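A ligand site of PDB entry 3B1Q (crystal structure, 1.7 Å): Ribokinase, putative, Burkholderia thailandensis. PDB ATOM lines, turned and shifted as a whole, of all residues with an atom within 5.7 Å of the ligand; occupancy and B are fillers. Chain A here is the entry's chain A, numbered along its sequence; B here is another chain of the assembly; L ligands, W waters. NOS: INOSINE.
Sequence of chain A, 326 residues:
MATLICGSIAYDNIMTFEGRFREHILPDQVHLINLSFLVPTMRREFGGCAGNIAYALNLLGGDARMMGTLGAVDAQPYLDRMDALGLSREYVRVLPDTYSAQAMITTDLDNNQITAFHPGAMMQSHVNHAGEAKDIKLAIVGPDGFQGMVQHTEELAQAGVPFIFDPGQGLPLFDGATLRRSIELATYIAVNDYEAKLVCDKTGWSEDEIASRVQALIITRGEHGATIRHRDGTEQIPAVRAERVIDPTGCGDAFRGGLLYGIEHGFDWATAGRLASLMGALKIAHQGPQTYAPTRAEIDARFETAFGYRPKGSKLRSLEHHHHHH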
ATOM      1  N   SER A   8     -17.061  -6.621 -11.494  1.00  0.00           N
ATOM      2  CA  SER A   8     -16.684  -7.440 -12.665  1.00  0.00           C
ATOM      3  C   SER A   8     -15.393  -6.914 -13.321  1.00  0.00           C
ATOM      4  O   SER A   8     -15.080  -5.730 -13.260  1.00  0.00           O
ATOM      5  CB  SER A   8     -17.835  -7.518 -13.718  1.00  0.00           C
ATOM      6  OG  SER A   8     -18.223  -6.231 -14.130  1.00  0.00           O
ATOM      7  N   ALA A  10     -13.863  -7.471 -17.204  1.00  0.00           N
ATOM      8  CA  ALA A  10     -14.477  -8.071 -18.380  1.00  0.00           C
ATOM      9  C   ALA A  10     -13.919  -7.426 -19.649  1.00  0.00           C
ATOM     10  O   ALA A  10     -13.432  -6.283 -19.612  1.00  0.00           O
ATOM     11  CB  ALA A  10     -16.027  -7.827 -18.352  1.00  0.00           C
ATOM     12  N   TYR A  11     -14.017  -8.150 -20.754  1.00  0.00           N
ATOM     13  CA  TYR A  11     -13.752  -7.545 -22.023  1.00  0.00           C
ATOM     14  C   TYR A  11     -15.059  -7.162 -22.665  1.00  0.00           C
ATOM     15  O   TYR A  11     -15.985  -8.010 -22.721  1.00  0.00           O
ATOM     16  CB  TYR A  11     -13.043  -8.532 -22.918  1.00  0.00           C
ATOM     17  CG  TYR A  11     -11.693  -8.917 -22.340  1.00  0.00           C
ATOM     18  CD1 TYR A  11     -10.657  -7.982 -22.263  1.00  0.00           C
ATOM     19  CD2 TYR A  11     -11.446 -10.220 -21.936  1.00  0.00           C
ATOM     20  CE1 TYR A  11      -9.387  -8.361 -21.743  1.00  0.00           C
ATOM     21  CE2 TYR A  11     -10.193 -10.635 -21.394  1.00  0.00           C
ATOM     22  CZ  TYR A  11      -9.167  -9.687 -21.332  1.00  0.00           C
ATOM     23  OH  TYR A  11      -7.923 -10.021 -20.836  1.00  0.00           O
ATOM     24  N   ASP A  12     -15.115  -5.922 -23.174  1.00  0.00           N
ATOM     25  CA  ASP A  12     -16.349  -5.381 -23.744  1.00  0.00           C
ATOM     26  C   ASP A  12     -16.293  -5.402 -25.260  1.00  0.00           C
ATOM     27  O   ASP A  12     -15.256  -5.113 -25.855  1.00  0.00           O
ATOM     28  CB  ASP A  12     -16.631  -3.940 -23.279  1.00  0.00           C
ATOM     29  CG  ASP A  12     -17.002  -3.838 -21.812  1.00  0.00           C
ATOM     30  OD1 ASP A  12     -17.300  -4.850 -21.140  1.00  0.00           O
ATOM     31  OD2 ASP A  12     -17.027  -2.694 -21.361  1.00  0.00           O
ATOM     32  N   PHE A  46     -11.274  -2.754 -22.966  1.00  0.00           N
ATOM     33  CA  PHE A  46     -11.203  -3.203 -21.587  1.00  0.00           C
ATOM     34  C   PHE A  46     -12.337  -2.655 -20.774  1.00  0.00           C
ATOM     35  O   PHE A  46     -12.683  -1.445 -20.852  1.00  0.00           O
ATOM     36  CB  PHE A  46      -9.871  -2.775 -20.976  1.00  0.00           C
ATOM     37  CG  PHE A  46      -8.692  -3.409 -21.621  1.00  0.00           C
ATOM     38  CD1 PHE A  46      -8.242  -4.685 -21.224  1.00  0.00           C
ATOM     39  CD2 PHE A  46      -7.988  -2.705 -22.622  1.00  0.00           C
ATOM     40  CE1 PHE A  46      -7.116  -5.240 -21.828  1.00  0.00           C
ATOM     41  CE2 PHE A  46      -6.864  -3.268 -23.231  1.00  0.00           C
ATOM     42  CZ  PHE A  46      -6.439  -4.535 -22.822  1.00  0.00           C
ATOM     43  N   GLY A  47     -12.950  -3.559 -19.973  1.00  0.00           N
ATOM     44  CA  GLY A  47     -14.190  -3.135 -19.253  1.00  0.00           C
ATOM     45  C   GLY A  47     -14.361  -3.893 -17.965  1.00  0.00           C
ATOM     46  O   GLY A  47     -13.369  -4.321 -17.330  1.00  0.00           O
ATOM     47  N   GLY A  48     -15.625  -4.108 -17.630  1.00  0.00           N
ATOM     48  CA  GLY A  48     -15.934  -4.625 -16.279  1.00  0.00           C
ATOM     49  C   GLY A  48     -16.031  -3.454 -15.253  1.00  0.00           C
ATOM     50  O   GLY A  48     -15.200  -2.542 -15.210  1.00  0.00           O
ATOM     51  N   CYS A  49     -16.999  -3.552 -14.366  1.00  0.00           N
ATOM     52  CA  CYS A  49     -17.240  -2.476 -13.448  1.00  0.00           C
ATOM     53  C   CYS A  49     -16.034  -2.169 -12.586  1.00  0.00           C
ATOM     54  O   CYS A  49     -15.701  -0.993 -12.376  1.00  0.00           O
ATOM     55  CB  CYS A  49     -18.464  -2.827 -12.565  1.00  0.00           C
ATOM     56  SG  CYS A  49     -19.945  -3.095 -13.604  1.00  0.00           S
ATOM     57  N   ASN A  52     -13.214  -0.512 -14.709  1.00  0.00           N
ATOM     58  CA  ASN A  52     -13.629   0.845 -15.090  1.00  0.00           C
ATOM     59  C   ASN A  52     -13.552   1.803 -13.892  1.00  0.00           C
ATOM     60  O   ASN A  52     -12.994   2.914 -14.009  1.00  0.00           O
ATOM     61  CB  ASN A  52     -15.101   0.801 -15.579  1.00  0.00           C
ATOM     62  CG  ASN A  52     -15.272   0.013 -16.856  1.00  0.00           C
ATOM     63  OD1 ASN A  52     -14.301  -0.358 -17.523  1.00  0.00           O
ATOM     64  ND2 ASN A  52     -16.531  -0.293 -17.182  1.00  0.00           N
ATOM     65  N   ALA A 103     -18.706  -8.800 -22.226  1.00  0.00           N
ATOM     66  CA  ALA A 103     -19.971  -8.100 -22.462  1.00  0.00           C
ATOM     67  C   ALA A 103     -20.135  -7.886 -23.955  1.00  0.00           C
ATOM     68  O   ALA A 103     -19.192  -7.406 -24.603  1.00  0.00           O
ATOM     69  CB  ALA A 103     -20.000  -6.762 -21.719  1.00  0.00           C
ATOM     70  N   ILE A 105     -22.231  -5.604 -26.117  1.00  0.00           N
ATOM     71  CA  ILE A 105     -22.943  -4.364 -25.721  1.00  0.00           C
ATOM     72  C   ILE A 105     -23.377  -3.630 -26.982  1.00  0.00           C
ATOM     73  O   ILE A 105     -22.559  -3.357 -27.850  1.00  0.00           O
ATOM     74  CB  ILE A 105     -22.023  -3.396 -24.921  1.00  0.00           C
ATOM     75  CG1 ILE A 105     -21.487  -4.034 -23.613  1.00  0.00           C
ATOM     76  CG2 ILE A 105     -22.762  -2.057 -24.590  1.00  0.00           C
ATOM     77  CD1 ILE A 105     -20.444  -3.094 -22.843  1.00  0.00           C
ATOM     78  N   THR A 115     -27.270  -5.323 -23.295  1.00  0.00           N
ATOM     79  CA  THR A 115     -26.029  -6.133 -23.178  1.00  0.00           C
ATOM     80  C   THR A 115     -26.355  -7.617 -22.956  1.00  0.00           C
ATOM     81  O   THR A 115     -27.211  -7.922 -22.121  1.00  0.00           O
ATOM     82  CB  THR A 115     -25.161  -5.594 -22.057  1.00  0.00           C
ATOM     83  OG1 THR A 115     -24.776  -4.251 -22.376  1.00  0.00           O
ATOM     84  CG2 THR A 115     -23.872  -6.482 -21.821  1.00  0.00           C
ATOM     85  N   PHE A 117     -24.422 -10.498 -21.307  1.00  0.00           N
ATOM     86  CA  PHE A 117     -23.184 -10.544 -20.512  1.00  0.00           C
ATOM     87  C   PHE A 117     -22.832 -11.989 -20.198  1.00  0.00           C
ATOM     88  O   PHE A 117     -23.614 -12.686 -19.582  1.00  0.00           O
ATOM     89  CB  PHE A 117     -23.353  -9.758 -19.224  1.00  0.00           C
ATOM     90  CG  PHE A 117     -22.070  -9.581 -18.482  1.00  0.00           C
ATOM     91  CD1 PHE A 117     -21.195  -8.562 -18.842  1.00  0.00           C
ATOM     92  CD2 PHE A 117     -21.717 -10.404 -17.427  1.00  0.00           C
ATOM     93  CE1 PHE A 117     -19.996  -8.354 -18.121  1.00  0.00           C
ATOM     94  CE2 PHE A 117     -20.494 -10.217 -16.753  1.00  0.00           C
ATOM     95  CZ  PHE A 117     -19.662  -9.206 -17.108  1.00  0.00           C
ATOM     96  N   MET A 122     -16.375 -14.509 -13.616  1.00  0.00           N
ATOM     97  CA  MET A 122     -17.132 -13.722 -12.686  1.00  0.00           C
ATOM     98  C   MET A 122     -18.029 -14.548 -11.775  1.00  0.00           C
ATOM     99  O   MET A 122     -18.251 -14.141 -10.634  1.00  0.00           O
ATOM    100  CB  MET A 122     -17.960 -12.662 -13.449  1.00  0.00           C
ATOM    101  CG  MET A 122     -18.566 -11.638 -12.496  1.00  0.00           C
ATOM    102  SD  MET A 122     -19.738 -10.479 -13.307  1.00  0.00           S
ATOM    103  CE  MET A 122     -21.208 -11.500 -13.422  1.00  0.00           C
ATOM    104  N   PRO A 143     -21.539  -4.472  -9.687  1.00  0.00           N
ATOM    105  CA  PRO A 143     -22.108  -5.637 -10.333  1.00  0.00           C
ATOM    106  C   PRO A 143     -21.057  -6.734 -10.514  1.00  0.00           C
ATOM    107  O   PRO A 143     -19.932  -6.483 -10.952  1.00  0.00           O
ATOM    108  CB  PRO A 143     -22.661  -5.084 -11.673  1.00  0.00           C
ATOM    109  CG  PRO A 143     -22.864  -3.606 -11.429  1.00  0.00           C
ATOM    110  CD  PRO A 143     -21.753  -3.218 -10.461  1.00  0.00           C
ATOM    111  N   ASP A 144     -21.429  -7.942 -10.127  1.00  0.00           N
ATOM    112  CA  ASP A 144     -20.450  -9.030  -9.977  1.00  0.00           C
ATOM    113  C   ASP A 144     -21.248 -10.310  -9.956  1.00  0.00           C
ATOM    114  O   ASP A 144     -22.455 -10.319 -10.194  1.00  0.00           O
ATOM    115  CB  ASP A 144     -19.687  -8.822  -8.646  1.00  0.00           C
ATOM    116  CG  ASP A 144     -18.238  -9.284  -8.704  1.00  0.00           C
ATOM    117  OD1 ASP A 144     -17.957 -10.188  -9.543  1.00  0.00           O
ATOM    118  OD2 ASP A 144     -17.381  -8.763  -7.930  1.00  0.00           O
ATOM    119  N   GLN A 169     -26.264  -3.692 -12.908  1.00  0.00           N
ATOM    120  CA  GLN A 169     -26.730  -4.849 -13.704  1.00  0.00           C
ATOM    121  C   GLN A 169     -26.982  -6.118 -12.901  1.00  0.00           C
ATOM    122  O   GLN A 169     -27.703  -7.024 -13.363  1.00  0.00           O
ATOM    123  CB  GLN A 169     -25.695  -5.155 -14.808  1.00  0.00           C
ATOM    124  CG  GLN A 169     -25.576  -4.043 -15.811  1.00  0.00           C
ATOM    125  CD  GLN A 169     -24.370  -3.180 -15.532  1.00  0.00           C
ATOM    126  OE1 GLN A 169     -23.970  -3.028 -14.375  1.00  0.00           O
ATOM    127  NE2 GLN A 169     -23.749  -2.617 -16.590  1.00  0.00           N
ATOM    128  N   GLY A 170     -26.424  -6.178 -11.693  1.00  0.00           N
ATOM    129  CA  GLY A 170     -26.743  -7.229 -10.743  1.00  0.00           C
ATOM    130  C   GLY A 170     -28.099  -7.198 -10.060  1.00  0.00           C
ATOM    131  O   GLY A 170     -28.518  -8.190  -9.472  1.00  0.00           O
ATOM    132  N   THR A 249     -20.918   3.797 -22.827  1.00  0.00           N
ATOM    133  CA  THR A 249     -20.440   2.641 -22.056  1.00  0.00           C
ATOM    134  C   THR A 249     -19.390   3.007 -21.038  1.00  0.00           C
ATOM    135  O   THR A 249     -18.315   3.464 -21.404  1.00  0.00           O
ATOM    136  CB  THR A 249     -19.829   1.539 -22.951  1.00  0.00           C
ATOM    137  OG1 THR A 249     -20.690   1.270 -24.074  1.00  0.00           O
ATOM    138  CG2 THR A 249     -19.496   0.274 -22.104  1.00  0.00           C
ATOM    139  N   GLY A 250     -19.718   2.797 -19.772  1.00  0.00           N
ATOM    140  CA  GLY A 250     -18.788   3.129 -18.671  1.00  0.00           C
ATOM    141  C   GLY A 250     -18.963   4.511 -18.060  1.00  0.00           C
ATOM    142  O   GLY A 250     -18.190   4.876 -17.159  1.00  0.00           O
ATOM    143  N   ASP A 253     -19.554   4.215 -14.342  1.00  0.00           N
ATOM    144  CA  ASP A 253     -18.365   3.873 -13.619  1.00  0.00           C
ATOM    145  C   ASP A 253     -17.369   4.993 -13.461  1.00  0.00           C
ATOM    146  O   ASP A 253     -16.735   5.114 -12.414  1.00  0.00           O
ATOM    147  CB  ASP A 253     -17.693   2.640 -14.303  1.00  0.00           C
ATOM    148  CG  ASP A 253     -18.572   1.391 -14.233  1.00  0.00           C
ATOM    149  OD1 ASP A 253     -19.436   1.320 -13.307  1.00  0.00           O
ATOM    150  OD2 ASP A 253     -18.463   0.491 -15.120  1.00  0.00           O
ATOM    151  N   PRO A 289     -15.131   2.058 -22.117  1.00  0.00           N
ATOM    152  CA  PRO A 289     -15.132   2.647 -20.804  1.00  0.00           C
ATOM    153  C   PRO A 289     -13.842   3.325 -20.367  1.00  0.00           C
ATOM    154  O   PRO A 289     -13.914   4.126 -19.435  1.00  0.00           O
ATOM    155  CB  PRO A 289     -15.415   1.470 -19.839  1.00  0.00           C
ATOM    156  CG  PRO A 289     -15.777   0.338 -20.719  1.00  0.00           C
ATOM    157  CD  PRO A 289     -15.285   0.596 -22.121  1.00  0.00           C
ATOM    158  N   ASN B  34     -30.232   0.927 -19.360  1.00  0.00           N
ATOM    159  CA  ASN B  34     -28.952   0.250 -19.430  1.00  0.00           C
ATOM    160  C   ASN B  34     -29.088  -1.234 -18.993  1.00  0.00           C
ATOM    161  O   ASN B  34     -28.654  -1.610 -17.898  1.00  0.00           O
ATOM    162  CB  ASN B  34     -27.961   1.028 -18.553  1.00  0.00           C
ATOM    163  CG  ASN B  34     -26.511   0.610 -18.765  1.00  0.00           C
ATOM    164  OD1 ASN B  34     -26.131   0.134 -19.848  1.00  0.00           O
ATOM    165  ND2 ASN B  34     -25.680   0.819 -17.724  1.00  0.00           N
ATOM    166  N   SER B  36     -28.733  -5.398 -19.024  1.00  0.00           N
ATOM    167  CA  SER B  36     -27.986  -6.655 -19.334  1.00  0.00           C
ATOM    168  C   SER B  36     -28.787  -7.913 -19.057  1.00  0.00           C
ATOM    169  O   SER B  36     -29.595  -7.981 -18.115  1.00  0.00           O
ATOM    170  CB  SER B  36     -26.635  -6.773 -18.572  1.00  0.00           C
ATOM    171  OG  SER B  36     -26.028  -5.531 -18.321  1.00  0.00           O
ATOM    172  N   LEU B  38     -27.856 -11.909 -18.472  1.00  0.00           N
ATOM    173  CA  LEU B  38     -26.825 -12.892 -18.239  1.00  0.00           C
ATOM    174  C   LEU B  38     -26.964 -14.095 -19.149  1.00  0.00           C
ATOM    175  O   LEU B  38     -28.053 -14.670 -19.309  1.00  0.00           O
ATOM    176  CB  LEU B  38     -26.907 -13.341 -16.800  1.00  0.00           C
ATOM    177  CG  LEU B  38     -25.726 -13.330 -15.855  1.00  0.00           C
ATOM    178  CD1 LEU B  38     -24.943 -12.016 -15.759  1.00  0.00           C
ATOM    179  CD2 LEU B  38     -26.343 -13.667 -14.536  1.00  0.00           C
HETATM  180  N9  NOS L   1     -21.241  -5.286 -17.234  1.00  0.00           N
HETATM  181  C4  NOS L   1     -21.484  -6.097 -16.208  1.00  0.00           C
HETATM  182  N3  NOS L   1     -20.800  -6.435 -15.078  1.00  0.00           N
HETATM  183  C2  NOS L   1     -21.335  -7.308 -14.200  1.00  0.00           C
HETATM  184  N1  NOS L   1     -22.539  -7.872 -14.415  1.00  0.00           N
HETATM  185  C6  NOS L   1     -23.279  -7.622 -15.526  1.00  0.00           C
HETATM  186  O6  NOS L   1     -24.455  -8.187 -15.747  1.00  0.00           O
HETATM  187  C5  NOS L   1     -22.791  -6.687 -16.516  1.00  0.00           C
HETATM  188  N7  NOS L   1     -23.222  -6.157 -17.678  1.00  0.00           N
HETATM  189  C8  NOS L   1     -22.266  -5.304 -18.104  1.00  0.00           C
HETATM  190  C5' NOS L   1     -20.267  -0.722 -17.595  1.00  0.00           C
HETATM  191  O5' NOS L   1     -20.574  -0.291 -16.233  1.00  0.00           O
HETATM  192  C4' NOS L   1     -19.622  -2.107 -17.435  1.00  0.00           C
HETATM  193  O4' NOS L   1     -20.579  -3.130 -16.991  1.00  0.00           O
HETATM  194  C1' NOS L   1     -20.027  -4.418 -17.289  1.00  0.00           C
HETATM  195  C2' NOS L   1     -19.426  -4.204 -18.657  1.00  0.00           C
HETATM  196  O2' NOS L   1     -18.318  -5.106 -18.746  1.00  0.00           O
HETATM  197  C3' NOS L   1     -19.097  -2.727 -18.743  1.00  0.00           C
HETATM  198  O3' NOS L   1     -17.703  -2.450 -18.972  1.00  0.00           O
HETATM  199  O   HOH W   1     -20.935   2.468 -16.295  1.00  0.00           O
HETATM  200  O   HOH W   2     -23.201  -0.751 -14.395  1.00  0.00           O
HETATM  201  O   HOH W   3     -26.060  -9.609 -13.685  1.00  0.00           O
HETATM  202  O   HOH W   4     -23.846  -9.016 -12.235  1.00  0.00           O
HETATM  203  O   HOH W   5     -22.926  -3.013 -20.167  1.00  0.00           O
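An oxygen (O3') of the ligand is in hydrogen-bond range of the side-chain carboxylate of Asp 12, 2.5 Å away.
The side-chain hydroxyl (OG) of Ser 36 of chain B lies within hydrogen-bond range of a nitrogen (N7) of the ligand (2.9 Å).
An oxygen (O3') of the ligand lies within hydrogen-bond range of the backbone NH (N) of Gly 48, at 3.0 Å.
NE2 of Gln 169 is in hydrogen-bond range of O4' of the ligand, 3.2 Å away.
SG of Cys 49 lies within hydrogen-bond range of O4' of the ligand.
The side-chain hydroxyl (OG) of Ser 8 sits at hydrogen-bond distance from a nitrogen (N3) of the ligand.
The side-chain amide nitrogen of Asn 52 lies within hydrogen-bond range of an oxygen (O3') of the ligand, 3.0 Å away.
O5' of the ligand is in hydrogen-bond range of OD2 of Asp 253.
The side-chain hydroxyl (OG) of Ser 8 sits at hydrogen-bond distance from the backbone NH (N) of Cys 49 (3.0 Å).
ND2 of Asn 52 sits close to O of Gly 48, at 3.3 Å.
The backbone NH (N) of Ser 8 sits at hydrogen-bond distance from the backbone carbonyl oxygen (O) of Pro 143.
ND2 of Asn 52 lies within hydrogen-bond range of OD2 of Asp 253 (2.9 Å).
The backbone NH (N) of Ala 103 sits at hydrogen-bond distance from the backbone carbonyl oxygen (O) of Tyr 11.
The backbone carbonyl oxygen (O) of Ala 10 sits at hydrogen-bond distance from the backbone NH (N) of Gly 47, 2.8 Å away.
CB of Ala 10 touches O2' of the ligand, 3.6 Å away.
Gly 47 touches the ligand.
Ala 103 touches the ligand (CB to O2', 3.8 Å).
Phe 117 touches the ligand (CE1 to C4, 3.3 Å).
Met 122 touches the ligand (SD to C2, 3.7 Å).
CB of Pro 143 touches C2 of the ligand (3.6 Å).
CG of Pro 289 touches O3' of the ligand, at 3.8 Å.
Leu 38 of chain B touches the ligand (CD1 to O6, 3.9 Å).
Hydrophobic or aromatic side chains within 4 Å of the ligand: Ala 10, Ala 103, Phe 117, Met 122, Pro 143, Pro 289 and Leu 38 of chain B.
Within 4 Å of the ligand: Ser 8, Ala 10, Asp 12, Gly 47, Gly 48, Cys 49, Asn 52, Ala 103, Phe 117, Met 122, Pro 143, Gln 169, Asp 253, Pro 289, Ser 36 of chain B and Leu 38 of chain B.
Water W1 lies within hydrogen-bond range of an oxygen (O5') of the ligand (2.8 Å) and the backbone NH (N) of Asp 253 (3.0 Å).
Water W4 bridges a nitrogen (N1) of the ligand (2.8 Å) and the backbone carbonyl oxygen of Asp 144 (2.8 Å).
Water W3 lies within hydrogen-bond range of an oxygen (O6) of the ligand (3.0 Å) and the backbone carbonyl oxygen of Gln 169 (3.1 Å).
Water W2 bridges the side-chain amide oxygen of Gln 169 (2.4 Å) and an oxygen (O5') of the ligand (3.2 Å).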
